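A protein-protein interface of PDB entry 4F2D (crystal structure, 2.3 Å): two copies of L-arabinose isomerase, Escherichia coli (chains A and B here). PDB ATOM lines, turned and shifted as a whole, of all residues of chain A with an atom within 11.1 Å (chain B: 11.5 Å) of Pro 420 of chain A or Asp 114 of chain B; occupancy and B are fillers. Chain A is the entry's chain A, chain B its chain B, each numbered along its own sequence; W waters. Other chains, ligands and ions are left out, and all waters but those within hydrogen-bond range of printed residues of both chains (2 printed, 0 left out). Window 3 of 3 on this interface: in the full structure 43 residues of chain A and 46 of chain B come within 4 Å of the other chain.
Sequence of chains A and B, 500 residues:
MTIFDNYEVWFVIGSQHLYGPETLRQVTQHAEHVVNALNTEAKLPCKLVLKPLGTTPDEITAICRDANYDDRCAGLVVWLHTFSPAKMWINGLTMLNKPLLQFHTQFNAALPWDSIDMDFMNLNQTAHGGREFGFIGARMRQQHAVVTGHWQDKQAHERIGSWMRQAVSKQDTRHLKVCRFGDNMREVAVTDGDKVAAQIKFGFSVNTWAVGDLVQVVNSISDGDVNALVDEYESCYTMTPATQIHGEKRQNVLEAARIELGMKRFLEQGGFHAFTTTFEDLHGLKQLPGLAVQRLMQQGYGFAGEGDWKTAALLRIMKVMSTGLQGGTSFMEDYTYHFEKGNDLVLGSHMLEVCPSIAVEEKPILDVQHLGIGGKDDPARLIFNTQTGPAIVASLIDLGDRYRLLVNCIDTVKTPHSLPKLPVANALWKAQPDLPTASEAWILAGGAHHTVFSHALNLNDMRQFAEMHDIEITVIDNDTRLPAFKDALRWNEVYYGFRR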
ATOM      1  N   THR A 240       1.057  -0.792   7.539  1.00  0.00           N
ATOM      2  CA  THR A 240       0.806  -2.065   8.227  1.00  0.00           C
ATOM      3  C   THR A 240       0.326  -1.805   9.657  1.00  0.00           C
ATOM      4  O   THR A 240       0.605  -0.743  10.213  1.00  0.00           O
ATOM      5  CB  THR A 240       2.065  -2.957   8.283  1.00  0.00           C
ATOM      6  OG1 THR A 240       3.088  -2.304   9.043  1.00  0.00           O
ATOM      7  CG2 THR A 240       2.577  -3.268   6.880  1.00  0.00           C
ATOM      8  N   THR A 336      20.302 -12.380  -4.320  1.00  0.00           N
ATOM      9  CA  THR A 336      20.278 -13.842  -4.437  1.00  0.00           C
ATOM     10  C   THR A 336      19.761 -14.295  -5.799  1.00  0.00           C
ATOM     11  O   THR A 336      19.200 -13.498  -6.554  1.00  0.00           O
ATOM     12  CB  THR A 336      19.425 -14.480  -3.317  1.00  0.00           C
ATOM     13  OG1 THR A 336      19.668 -15.891  -3.265  1.00  0.00           O
ATOM     14  CG2 THR A 336      17.940 -14.220  -3.544  1.00  0.00           C
ATOM     15  N   HIS A 338      17.895 -17.436  -8.452  1.00  0.00           N
ATOM     16  CA  HIS A 338      16.990 -18.549  -8.659  1.00  0.00           C
ATOM     17  C   HIS A 338      17.532 -19.350  -9.802  1.00  0.00           C
ATOM     18  O   HIS A 338      17.506 -18.897 -10.942  1.00  0.00           O
ATOM     19  CB  HIS A 338      15.596 -18.036  -8.988  1.00  0.00           C
ATOM     20  CG  HIS A 338      14.578 -19.124  -9.225  1.00  0.00           C
ATOM     21  ND1 HIS A 338      13.796 -19.608  -8.248  1.00  0.00           N
ATOM     22  CD2 HIS A 338      14.213 -19.799 -10.388  1.00  0.00           C
ATOM     23  CE1 HIS A 338      12.978 -20.551  -8.751  1.00  0.00           C
ATOM     24  NE2 HIS A 338      13.236 -20.665 -10.063  1.00  0.00           N
ATOM     25  N   LEU A 347      17.436 -11.996  -8.032  1.00  0.00           N
ATOM     26  CA  LEU A 347      16.671 -11.150  -7.121  1.00  0.00           C
ATOM     27  C   LEU A 347      17.572 -10.022  -6.631  1.00  0.00           C
ATOM     28  O   LEU A 347      18.657 -10.265  -6.095  1.00  0.00           O
ATOM     29  CB  LEU A 347      16.113 -11.942  -5.936  1.00  0.00           C
ATOM     30  CG  LEU A 347      15.080 -11.177  -5.093  1.00  0.00           C
ATOM     31  CD1 LEU A 347      13.971 -12.075  -4.576  1.00  0.00           C
ATOM     32  CD2 LEU A 347      15.743 -10.464  -3.929  1.00  0.00           C
ATOM     33  N   ILE A 365       4.102  -0.652   0.620  1.00  0.00           N
ATOM     34  CA  ILE A 365       3.847  -0.949   2.014  1.00  0.00           C
ATOM     35  C   ILE A 365       4.906  -0.230   2.818  1.00  0.00           C
ATOM     36  O   ILE A 365       6.052  -0.163   2.398  1.00  0.00           O
ATOM     37  CB  ILE A 365       3.953  -2.456   2.302  1.00  0.00           C
ATOM     38  CG1 ILE A 365       2.782  -3.209   1.677  1.00  0.00           C
ATOM     39  CG2 ILE A 365       3.974  -2.724   3.797  1.00  0.00           C
ATOM     40  CD1 ILE A 365       2.951  -4.711   1.708  1.00  0.00           C
ATOM     41  N   ASP A 367       6.664  -0.439   6.442  1.00  0.00           N
ATOM     42  CA  ASP A 367       6.779  -1.379   7.543  1.00  0.00           C
ATOM     43  C   ASP A 367       8.034  -1.144   8.359  1.00  0.00           C
ATOM     44  O   ASP A 367       8.972  -0.499   7.896  1.00  0.00           O
ATOM     45  CB  ASP A 367       6.780  -2.809   6.990  1.00  0.00           C
ATOM     46  CG  ASP A 367       6.161  -3.807   7.942  1.00  0.00           C
ATOM     47  OD1 ASP A 367       6.754  -4.885   8.147  1.00  0.00           O
ATOM     48  OD2 ASP A 367       5.071  -3.527   8.480  1.00  0.00           O
ATOM     49  N   VAL A 368       8.026  -1.672   9.575  1.00  0.00           N
ATOM     50  CA  VAL A 368       9.165  -1.605  10.469  1.00  0.00           C
ATOM     51  C   VAL A 368       9.444  -3.019  10.923  1.00  0.00           C
ATOM     52  O   VAL A 368       8.551  -3.714  11.403  1.00  0.00           O
ATOM     53  CB  VAL A 368       8.890  -0.739  11.707  1.00  0.00           C
ATOM     54  CG1 VAL A 368      10.058  -0.799  12.680  1.00  0.00           C
ATOM     55  CG2 VAL A 368       8.617   0.695  11.300  1.00  0.00           C
ATOM     56  N   GLN A 369      10.674  -3.463  10.735  1.00  0.00           N
ATOM     57  CA  GLN A 369      11.086  -4.778  11.156  1.00  0.00           C
ATOM     58  C   GLN A 369      12.506  -4.742  11.597  1.00  0.00           C
ATOM     59  O   GLN A 369      13.161  -3.754  11.482  1.00  0.00           O
ATOM     60  CB  GLN A 369      10.987  -5.760  10.022  1.00  0.00           C
ATOM     61  CG  GLN A 369       9.596  -5.962   9.513  1.00  0.00           C
ATOM     62  CD  GLN A 369       9.159  -7.386   9.645  1.00  0.00           C
ATOM     63  OE1 GLN A 369       9.901  -8.231  10.109  1.00  0.00           O
ATOM     64  NE2 GLN A 369       7.953  -7.656   9.231  1.00  0.00           N
ATOM     65  N   ARG A 381      10.798   1.129   6.468  1.00  0.00           N
ATOM     66  CA  ARG A 381      11.136   1.009   5.050  1.00  0.00           C
ATOM     67  C   ARG A 381       9.890   0.844   4.192  1.00  0.00           C
ATOM     68  O   ARG A 381       8.823   0.489   4.693  1.00  0.00           O
ATOM     69  CB  ARG A 381      12.113  -0.152   4.810  1.00  0.00           C
ATOM     70  CG  ARG A 381      11.481  -1.525   4.581  1.00  0.00           C
ATOM     71  CD  ARG A 381      10.703  -2.024   5.785  1.00  0.00           C
ATOM     72  NE  ARG A 381      11.501  -2.018   7.006  1.00  0.00           N
ATOM     73  CZ  ARG A 381      12.452  -2.903   7.304  1.00  0.00           C
ATOM     74  NH1 ARG A 381      12.759  -3.892   6.472  1.00  0.00           N
ATOM     75  NH2 ARG A 381      13.111  -2.797   8.452  1.00  0.00           N
ATOM     76  N   ILE A 383       8.205  -1.331   1.262  1.00  0.00           N
ATOM     77  CA  ILE A 383       8.249  -2.641   0.615  1.00  0.00           C
ATOM     78  C   ILE A 383       7.373  -2.614  -0.634  1.00  0.00           C
ATOM     79  O   ILE A 383       6.239  -2.135  -0.597  1.00  0.00           O
ATOM     80  CB  ILE A 383       7.764  -3.756   1.561  1.00  0.00           C
ATOM     81  CG1 ILE A 383       8.597  -3.762   2.845  1.00  0.00           C
ATOM     82  CG2 ILE A 383       7.854  -5.118   0.873  1.00  0.00           C
ATOM     83  CD1 ILE A 383       8.121  -4.734   3.902  1.00  0.00           C
ATOM     84  N   PHE A 384       7.911  -3.121  -1.739  1.00  0.00           N
ATOM     85  CA  PHE A 384       7.215  -3.114  -3.027  1.00  0.00           C
ATOM     86  C   PHE A 384       7.882  -4.031  -4.051  1.00  0.00           C
ATOM     87  O   PHE A 384       9.047  -4.405  -3.911  1.00  0.00           O
ATOM     88  CB  PHE A 384       7.137  -1.692  -3.605  1.00  0.00           C
ATOM     89  CG  PHE A 384       8.470  -0.987  -3.694  1.00  0.00           C
ATOM     90  CD1 PHE A 384       9.317  -1.182  -4.780  1.00  0.00           C
ATOM     91  CD2 PHE A 384       8.871  -0.115  -2.693  1.00  0.00           C
ATOM     92  CE1 PHE A 384      10.538  -0.531  -4.855  1.00  0.00           C
ATOM     93  CE2 PHE A 384      10.088   0.542  -2.763  1.00  0.00           C
ATOM     94  CZ  PHE A 384      10.925   0.334  -3.844  1.00  0.00           C
ATOM     95  N   ASN A 385       7.120  -4.383  -5.079  1.00  0.00           N
ATOM     96  CA  ASN A 385       7.639  -5.096  -6.242  1.00  0.00           C
ATOM     97  C   ASN A 385       8.072  -4.109  -7.316  1.00  0.00           C
ATOM     98  O   ASN A 385       7.637  -2.958  -7.322  1.00  0.00           O
ATOM     99  CB  ASN A 385       6.586  -6.054  -6.799  1.00  0.00           C
ATOM    100  CG  ASN A 385       6.131  -7.065  -5.768  1.00  0.00           C
ATOM    101  OD1 ASN A 385       6.948  -7.743  -5.144  1.00  0.00           O
ATOM    102  ND2 ASN A 385       4.824  -7.157  -5.568  1.00  0.00           N
ATOM    103  N   THR A 415       7.277 -11.439  -9.959  1.00  0.00           N
ATOM    104  CA  THR A 415       7.510 -12.506  -8.987  1.00  0.00           C
ATOM    105  C   THR A 415       6.456 -13.599  -9.183  1.00  0.00           C
ATOM    106  O   THR A 415       5.262 -13.295  -9.259  1.00  0.00           O
ATOM    107  CB  THR A 415       7.438 -11.997  -7.535  1.00  0.00           C
ATOM    108  OG1 THR A 415       6.141 -11.451  -7.274  1.00  0.00           O
ATOM    109  CG2 THR A 415       8.495 -10.933  -7.278  1.00  0.00           C
ATOM    110  N   PRO A 416       6.888 -14.871  -9.265  1.00  0.00           N
ATOM    111  CA  PRO A 416       5.949 -15.969  -9.522  1.00  0.00           C
ATOM    112  C   PRO A 416       5.099 -16.323  -8.303  1.00  0.00           C
ATOM    113  O   PRO A 416       4.068 -16.980  -8.436  1.00  0.00           O
ATOM    114  CB  PRO A 416       6.872 -17.133  -9.895  1.00  0.00           C
ATOM    115  CG  PRO A 416       8.129 -16.861  -9.148  1.00  0.00           C
ATOM    116  CD  PRO A 416       8.269 -15.362  -9.080  1.00  0.00           C
ATOM    117  N   HIS A 417       5.557 -15.905  -7.128  1.00  0.00           N
ATOM    118  CA  HIS A 417       4.821 -16.083  -5.880  1.00  0.00           C
ATOM    119  C   HIS A 417       5.041 -14.881  -5.008  1.00  0.00           C
ATOM    120  O   HIS A 417       6.005 -14.157  -5.210  1.00  0.00           O
ATOM    121  CB  HIS A 417       5.329 -17.338  -5.197  1.00  0.00           C
ATOM    122  CG  HIS A 417       4.455 -17.834  -4.075  1.00  0.00           C
ATOM    123  ND1 HIS A 417       4.581 -17.395  -2.812  1.00  0.00           N
ATOM    124  CD2 HIS A 417       3.432 -18.781  -4.063  1.00  0.00           C
ATOM    125  CE1 HIS A 417       3.678 -18.020  -2.030  1.00  0.00           C
ATOM    126  NE2 HIS A 417       2.977 -18.870  -2.800  1.00  0.00           N
ATOM    127  N   SER A 418       4.162 -14.647  -4.036  1.00  0.00           N
ATOM    128  CA  SER A 418       4.369 -13.557  -3.065  1.00  0.00           C
ATOM    129  C   SER A 418       5.587 -13.796  -2.206  1.00  0.00           C
ATOM    130  O   SER A 418       5.971 -14.936  -2.022  1.00  0.00           O
ATOM    131  CB  SER A 418       3.173 -13.403  -2.135  1.00  0.00           C
ATOM    132  OG  SER A 418       2.820 -14.621  -1.500  1.00  0.00           O
ATOM    133  N   LEU A 419       6.183 -12.724  -1.681  1.00  0.00           N
ATOM    134  CA  LEU A 419       7.277 -12.845  -0.724  1.00  0.00           C
ATOM    135  C   LEU A 419       6.785 -12.255   0.594  1.00  0.00           C
ATOM    136  O   LEU A 419       7.055 -11.099   0.881  1.00  0.00           O
ATOM    137  CB  LEU A 419       8.545 -12.134  -1.233  1.00  0.00           C
ATOM    138  CG  LEU A 419       8.808 -12.229  -2.746  1.00  0.00           C
ATOM    139  CD1 LEU A 419      10.229 -11.813  -3.088  1.00  0.00           C
ATOM    140  CD2 LEU A 419       8.566 -13.631  -3.269  1.00  0.00           C
ATOM    141  N   PRO A 420       6.041 -13.047   1.393  1.00  0.00           N
ATOM    142  CA  PRO A 420       5.410 -12.503   2.602  1.00  0.00           C
ATOM    143  C   PRO A 420       6.371 -12.262   3.771  1.00  0.00           C
ATOM    144  O   PRO A 420       6.077 -11.437   4.635  1.00  0.00           O
ATOM    145  CB  PRO A 420       4.393 -13.585   2.975  1.00  0.00           C
ATOM    146  CG  PRO A 420       5.021 -14.847   2.499  1.00  0.00           C
ATOM    147  CD  PRO A 420       5.784 -14.492   1.252  1.00  0.00           C
ATOM    148  N   LYS A 421       7.495 -12.974   3.793  1.00  0.00           N
ATOM    149  CA  LYS A 421       8.474 -12.859   4.883  1.00  0.00           C
ATOM    150  C   LYS A 421       9.706 -12.021   4.530  1.00  0.00           C
ATOM    151  O   LYS A 421      10.616 -11.886   5.346  1.00  0.00           O
ATOM    152  CB  LYS A 421       8.904 -14.248   5.357  1.00  0.00           C
ATOM    153  CG  LYS A 421       7.765 -15.024   5.999  1.00  0.00           C
ATOM    154  CD  LYS A 421       8.254 -16.173   6.866  1.00  0.00           C
ATOM    155  CE  LYS A 421       7.204 -16.556   7.902  1.00  0.00           C
ATOM    156  NZ  LYS A 421       7.351 -17.964   8.366  1.00  0.00           N
ATOM    157  N   LEU A 422       9.730 -11.459   3.323  1.00  0.00           N
ATOM    158  CA  LEU A 422      10.832 -10.604   2.887  1.00  0.00           C
ATOM    159  C   LEU A 422      10.523  -9.151   3.260  1.00  0.00           C
ATOM    160  O   LEU A 422       9.677  -8.518   2.626  1.00  0.00           O
ATOM    161  CB  LEU A 422      11.047 -10.725   1.376  1.00  0.00           C
ATOM    162  CG  LEU A 422      12.367 -10.142   0.851  1.00  0.00           C
ATOM    163  CD1 LEU A 422      13.555 -10.966   1.316  1.00  0.00           C
ATOM    164  CD2 LEU A 422      12.345 -10.039  -0.669  1.00  0.00           C
ATOM    165  N   PRO A 423      11.222  -8.606   4.275  1.00  0.00           N
ATOM    166  CA  PRO A 423      10.866  -7.288   4.789  1.00  0.00           C
ATOM    167  C   PRO A 423      11.401  -6.113   3.961  1.00  0.00           C
ATOM    168  O   PRO A 423      11.316  -4.965   4.401  1.00  0.00           O
ATOM    169  CB  PRO A 423      11.513  -7.286   6.171  1.00  0.00           C
ATOM    170  CG  PRO A 423      12.747  -8.097   5.988  1.00  0.00           C
ATOM    171  CD  PRO A 423      12.412  -9.150   4.958  1.00  0.00           C
ATOM    172  N   VAL A 424      11.938  -6.392   2.776  1.00  0.00           N
ATOM    173  CA  VAL A 424      12.458  -5.344   1.899  1.00  0.00           C
ATOM    174  C   VAL A 424      11.842  -5.451   0.512  1.00  0.00           C
ATOM    175  O   VAL A 424      11.291  -6.491   0.140  1.00  0.00           O
ATOM    176  CB  VAL A 424      13.991  -5.420   1.765  1.00  0.00           C
ATOM    177  CG1 VAL A 424      14.651  -5.181   3.117  1.00  0.00           C
ATOM    178  CG2 VAL A 424      14.410  -6.764   1.182  1.00  0.00           C
ATOM    179  N   ALA A 425      11.947  -4.365  -0.248  1.00  0.00           N
ATOM    180  CA  ALA A 425      11.474  -4.340  -1.625  1.00  0.00           C
ATOM    181  C   ALA A 425      12.352  -5.237  -2.490  1.00  0.00           C
ATOM    182  O   ALA A 425      13.460  -5.618  -2.096  1.00  0.00           O
ATOM    183  CB  ALA A 425      11.463  -2.921  -2.171  1.00  0.00           C
ATOM    184  N   ASN A 426      11.849  -5.572  -3.671  1.00  0.00           N
ATOM    185  CA  ASN A 426      12.563  -6.470  -4.567  1.00  0.00           C
ATOM    186  C   ASN A 426      12.486  -6.056  -6.032  1.00  0.00           C
ATOM    187  O   ASN A 426      11.490  -5.493  -6.492  1.00  0.00           O
ATOM    188  CB  ASN A 426      12.045  -7.910  -4.403  1.00  0.00           C
ATOM    189  CG  ASN A 426      10.787  -8.175  -5.206  1.00  0.00           C
ATOM    190  OD1 ASN A 426      10.850  -8.458  -6.408  1.00  0.00           O
ATOM    191  ND2 ASN A 426       9.636  -8.090  -4.547  1.00  0.00           N
ATOM    192  N   ASN B 108      21.207 -23.577  -2.328  1.00  0.00           N
ATOM    193  CA  ASN B 108      19.914 -23.848  -2.951  1.00  0.00           C
ATOM    194  C   ASN B 108      19.920 -23.492  -4.419  1.00  0.00           C
ATOM    195  O   ASN B 108      20.575 -22.539  -4.833  1.00  0.00           O
ATOM    196  CB  ASN B 108      18.796 -23.060  -2.259  1.00  0.00           C
ATOM    197  CG  ASN B 108      18.971 -21.549  -2.385  1.00  0.00           C
ATOM    198  OD1 ASN B 108      20.024 -20.993  -2.042  1.00  0.00           O
ATOM    199  ND2 ASN B 108      17.935 -20.876  -2.884  1.00  0.00           N
ATOM    200  N   ALA B 110      16.633 -23.483  -6.228  1.00  0.00           N
ATOM    201  CA  ALA B 110      15.394 -22.715  -6.297  1.00  0.00           C
ATOM    202  C   ALA B 110      15.324 -21.694  -5.170  1.00  0.00           C
ATOM    203  O   ALA B 110      15.758 -21.958  -4.051  1.00  0.00           O
ATOM    204  CB  ALA B 110      14.190 -23.646  -6.231  1.00  0.00           C
ATOM    205  N   LEU B 111      14.755 -20.535  -5.479  1.00  0.00           N
ATOM    206  CA  LEU B 111      14.597 -19.448  -4.519  1.00  0.00           C
ATOM    207  C   LEU B 111      13.309 -19.670  -3.707  1.00  0.00           C
ATOM    208  O   LEU B 111      12.219 -19.710  -4.277  1.00  0.00           O
ATOM    209  CB  LEU B 111      14.581 -18.112  -5.268  1.00  0.00           C
ATOM    210  CG  LEU B 111      14.304 -16.786  -4.559  1.00  0.00           C
ATOM    211  CD1 LEU B 111      15.077 -16.706  -3.257  1.00  0.00           C
ATOM    212  CD2 LEU B 111      14.695 -15.625  -5.463  1.00  0.00           C
ATOM    213  N   PRO B 112      13.432 -19.837  -2.373  1.00  0.00           N
ATOM    214  CA  PRO B 112      12.259 -20.108  -1.525  1.00  0.00           C
ATOM    215  C   PRO B 112      11.347 -18.890  -1.376  1.00  0.00           C
ATOM    216  O   PRO B 112      11.400 -18.181  -0.371  1.00  0.00           O
ATOM    217  CB  PRO B 112      12.861 -20.516  -0.172  1.00  0.00           C
ATOM    218  CG  PRO B 112      14.292 -20.115  -0.204  1.00  0.00           C
ATOM    219  CD  PRO B 112      14.683 -19.743  -1.600  1.00  0.00           C
ATOM    220  N   TRP B 113      10.501 -18.681  -2.379  1.00  0.00           N
ATOM    221  CA  TRP B 113       9.689 -17.461  -2.487  1.00  0.00           C
ATOM    222  C   TRP B 113       8.861 -17.172  -1.260  1.00  0.00           C
ATOM    223  O   TRP B 113       8.751 -16.021  -0.834  1.00  0.00           O
ATOM    224  CB  TRP B 113       8.767 -17.535  -3.695  1.00  0.00           C
ATOM    225  CG  TRP B 113       9.467 -17.843  -4.999  1.00  0.00           C
ATOM    226  CD1 TRP B 113       9.483 -19.053  -5.682  1.00  0.00           C
ATOM    227  CD2 TRP B 113      10.265 -16.931  -5.830  1.00  0.00           C
ATOM    228  NE1 TRP B 113      10.217 -18.955  -6.833  1.00  0.00           N
ATOM    229  CE2 TRP B 113      10.712 -17.712  -6.982  1.00  0.00           C
ATOM    230  CE3 TRP B 113      10.643 -15.600  -5.734  1.00  0.00           C
ATOM    231  CZ2 TRP B 113      11.500 -17.164  -7.980  1.00  0.00           C
ATOM    232  CZ3 TRP B 113      11.436 -15.057  -6.747  1.00  0.00           C
ATOM    233  CH2 TRP B 113      11.853 -15.822  -7.843  1.00  0.00           C
ATOM    234  N   ASP B 114       8.277 -18.218  -0.683  1.00  0.00           N
ATOM    235  CA  ASP B 114       7.343 -18.075   0.444  1.00  0.00           C
ATOM    236  C   ASP B 114       7.994 -17.989   1.828  1.00  0.00           C
ATOM    237  O   ASP B 114       7.348 -17.561   2.779  1.00  0.00           O
ATOM    238  CB  ASP B 114       6.322 -19.223   0.442  1.00  0.00           C
ATOM    239  CG  ASP B 114       6.974 -20.590   0.335  1.00  0.00           C
ATOM    240  OD1 ASP B 114       8.064 -20.679  -0.283  1.00  0.00           O
ATOM    241  OD2 ASP B 114       6.391 -21.570   0.855  1.00  0.00           O
ATOM    242  N   SER B 115       9.250 -18.415   1.942  1.00  0.00           N
ATOM    243  CA  SER B 115       9.974 -18.380   3.224  1.00  0.00           C
ATOM    244  C   SER B 115      11.146 -17.393   3.263  1.00  0.00           C
ATOM    245  O   SER B 115      11.636 -17.053   4.346  1.00  0.00           O
ATOM    246  CB  SER B 115      10.483 -19.777   3.589  1.00  0.00           C
ATOM    247  OG  SER B 115      11.175 -20.369   2.511  1.00  0.00           O
ATOM    248  N   ILE B 116      11.600 -16.938   2.099  1.00  0.00           N
ATOM    249  CA  ILE B 116      12.786 -16.078   2.030  1.00  0.00           C
ATOM    250  C   ILE B 116      12.659 -14.847   2.941  1.00  0.00           C
ATOM    251  O   ILE B 116      11.676 -14.108   2.876  1.00  0.00           O
ATOM    252  CB  ILE B 116      13.123 -15.660   0.578  1.00  0.00           C
ATOM    253  CG1 ILE B 116      14.420 -14.844   0.547  1.00  0.00           C
ATOM    254  CG2 ILE B 116      11.974 -14.885  -0.050  1.00  0.00           C
ATOM    255  CD1 ILE B 116      15.023 -14.664  -0.831  1.00  0.00           C
ATOM    256  N   ASP B 117      13.661 -14.668   3.803  1.00  0.00           N
ATOM    257  CA  ASP B 117      13.715 -13.556   4.757  1.00  0.00           C
ATOM    258  C   ASP B 117      15.156 -13.040   4.918  1.00  0.00           C
ATOM    259  O   ASP B 117      16.065 -13.535   4.255  1.00  0.00           O
ATOM    260  CB  ASP B 117      13.121 -13.984   6.111  1.00  0.00           C
ATOM    261  CG  ASP B 117      13.839 -15.174   6.733  1.00  0.00           C
ATOM    262  OD1 ASP B 117      14.873 -15.621   6.199  1.00  0.00           O
ATOM    263  OD2 ASP B 117      13.355 -15.672   7.769  1.00  0.00           O
ATOM    264  N   MET B 118      15.361 -12.060   5.799  1.00  0.00           N
ATOM    265  CA  MET B 118      16.685 -11.422   5.973  1.00  0.00           C
ATOM    266  C   MET B 118      17.763 -12.373   6.417  1.00  0.00           C
ATOM    267  O   MET B 118      18.934 -12.216   6.042  1.00  0.00           O
ATOM    268  CB  MET B 118      16.615 -10.268   6.983  1.00  0.00           C
ATOM    269  CG  MET B 118      16.185  -8.965   6.321  1.00  0.00           C
ATOM    270  SD  MET B 118      17.414  -8.425   4.865  1.00  0.00           S
ATOM    271  CE  MET B 118      16.044  -8.443   3.451  1.00  0.00           C
ATOM    272  N   PHE B 120      17.990 -15.577   5.592  1.00  0.00           N
ATOM    273  CA  PHE B 120      18.371 -16.247   4.347  1.00  0.00           C
ATOM    274  C   PHE B 120      19.226 -15.330   3.457  1.00  0.00           C
ATOM    275  O   PHE B 120      20.193 -15.778   2.837  1.00  0.00           O
ATOM    276  CB  PHE B 120      17.123 -16.711   3.576  1.00  0.00           C
ATOM    277  CG  PHE B 120      17.441 -17.498   2.339  1.00  0.00           C
ATOM    278  CD1 PHE B 120      17.496 -18.886   2.377  1.00  0.00           C
ATOM    279  CD2 PHE B 120      17.720 -16.853   1.141  1.00  0.00           C
ATOM    280  CE1 PHE B 120      17.810 -19.612   1.246  1.00  0.00           C
ATOM    281  CE2 PHE B 120      18.038 -17.576   0.005  1.00  0.00           C
ATOM    282  CZ  PHE B 120      18.082 -18.958   0.057  1.00  0.00           C
ATOM    283  N   MET B 121      18.853 -14.053   3.405  1.00  0.00           N
ATOM    284  CA  MET B 121      19.556 -13.059   2.587  1.00  0.00           C
ATOM    285  C   MET B 121      20.938 -12.777   3.115  1.00  0.00           C
ATOM    286  O   MET B 121      21.857 -12.522   2.344  1.00  0.00           O
ATOM    287  CB  MET B 121      18.784 -11.739   2.546  1.00  0.00           C
ATOM    288  CG  MET B 121      17.455 -11.777   1.805  1.00  0.00           C
ATOM    289  SD  MET B 121      17.634 -11.942  -0.129  1.00  0.00           S
ATOM    290  CE  MET B 121      16.504 -10.429  -0.670  1.00  0.00           C
HETATM  291  O   HOH W   1       9.000 -14.272   1.752  1.00  0.00           O
HETATM  292  O   HOH W   2      18.076 -18.018  -3.504  1.00  0.00           O
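No position is printed for both chains.
Of the printed residues of chain B, Thr 336 of chain A touches Leu 111.
Ile 383 of chain A touches none of the printed residues of chain B.
His 417 of chain A touches just these residues of chain B: Trp 113 (3.8 Å) and Asp 114 (3.8 Å).
Pro 420 of chain A touches just these residues of chain B: Trp 113 and Asp 114.
Lys 421 of chain A touches just these residues of chain B: Ile 116 (3.3 Å) and Asp 117 (3.4 Å).
Asn 108 of chain B touches none of the printed residues of chain A.
No residue of chain A comes within 4 Å of Pro 112 of chain B.
Of chain A, only His 417 (3.8 Å) and Pro 420 (3.6 Å) come within 4 Å of Asp 114 of chain B.
Printed residues of chain A within 4 Å of Asp 117 of chain B: Lys 421.
The nearest residue of chain B that does not touch Pro 420 of chain A is Ser 115 of chain B (5.3 Å).
The backbone NH (N) of Leu 111 of chain B sits at hydrogen-bond distance from a ring nitrogen (ND1) of His 338 of chain A, 3.1 Å away.
N of Leu 422 of chain A sits at hydrogen-bond distance from O of Ile 116 of chain B (3.3 Å).
The backbone carbonyl oxygen (O) of Ser 418 of chain A lies close to the backbone carbonyl oxygen (O) of Trp 113 of chain B.
O of Lys 421 of chain A sits close to O of Ile 116 of chain B.
Water W2 lies within hydrogen-bond range of OG1 of Thr 336 of chain A (2.7 Å) and ND2 of Asn 108 of chain B (2.9 Å).
Water W1 lies within hydrogen-bond range of N of Lys 421 of chain A (2.8 Å), O of Ile 116 of chain B (2.9 Å), O of Trp 113 of chain B (3.1 Å) and N of Leu 422 of chain A (3.3 Å).
Of the 24 printed residues of chain A, 12 touch a printed residue of chain B.
Hydrophobic or aromatic side chains of chain A that line the printed part of chain B: His 338, Leu 347, Pro 416, His 417, Leu 419, Pro 420, Leu 422, Pro 423 and Val 424.
Hydrophobic or aromatic side chains of chain B within 4 Å of the printed part of chain A: Leu 111, Trp 113, Met 118 and Met 121.
Along chain B the printed residues that touch a printed residue of chain A span positions 111 to 121.
Among the printed residues, no Asp or Glu carboxylate lies within 4 Å of a Lys or Arg side-chain nitrogen of the other chain.
The backbone NH (N) of Leu 347 of chain A sits at hydrogen-bond distance from the backbone carbonyl oxygen (O) of Thr 336 of chain A (2.7 Å).
The guanidinium group (NH1) of Arg 381 of chain A sits at hydrogen-bond distance from the backbone carbonyl oxygen (O) of Pro 423 of chain A.
Among the printed residues, merely in contact across the chains: Thr 336 of chain A with Leu 111 of chain B (3.8 Å), His 338 of chain A with Trp 113 of chain B (3.4 Å), Leu 347 of chain A with Leu 111 of chain B (3.7 Å), Leu 347 of chain A with Met 121 of chain B (3.3 Å), Pro 416 of chain A with Trp 113 of chain B (3.5 Å), His 417 of chain A with Trp 113 of chain B (3.8 Å), His 417 of chain A with Asp 114 of chain B (3.8 Å), Leu 419 of chain A with Trp 113 of chain B (3.4 Å), Pro 420 of chain A with Trp 113 of chain B (3.9 Å), Pro 420 of chain A with Asp 114 of chain B (3.6 Å), Lys 421 of chain A with Asp 117 of chain B (3.4 Å), Leu 422 of chain A with Met 121 of chain B (3.6 Å), Pro 423 of chain A with Met 118 of chain B (3.6 Å) and Val 424 of chain A with Met 118 of chain B (3.3 Å).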
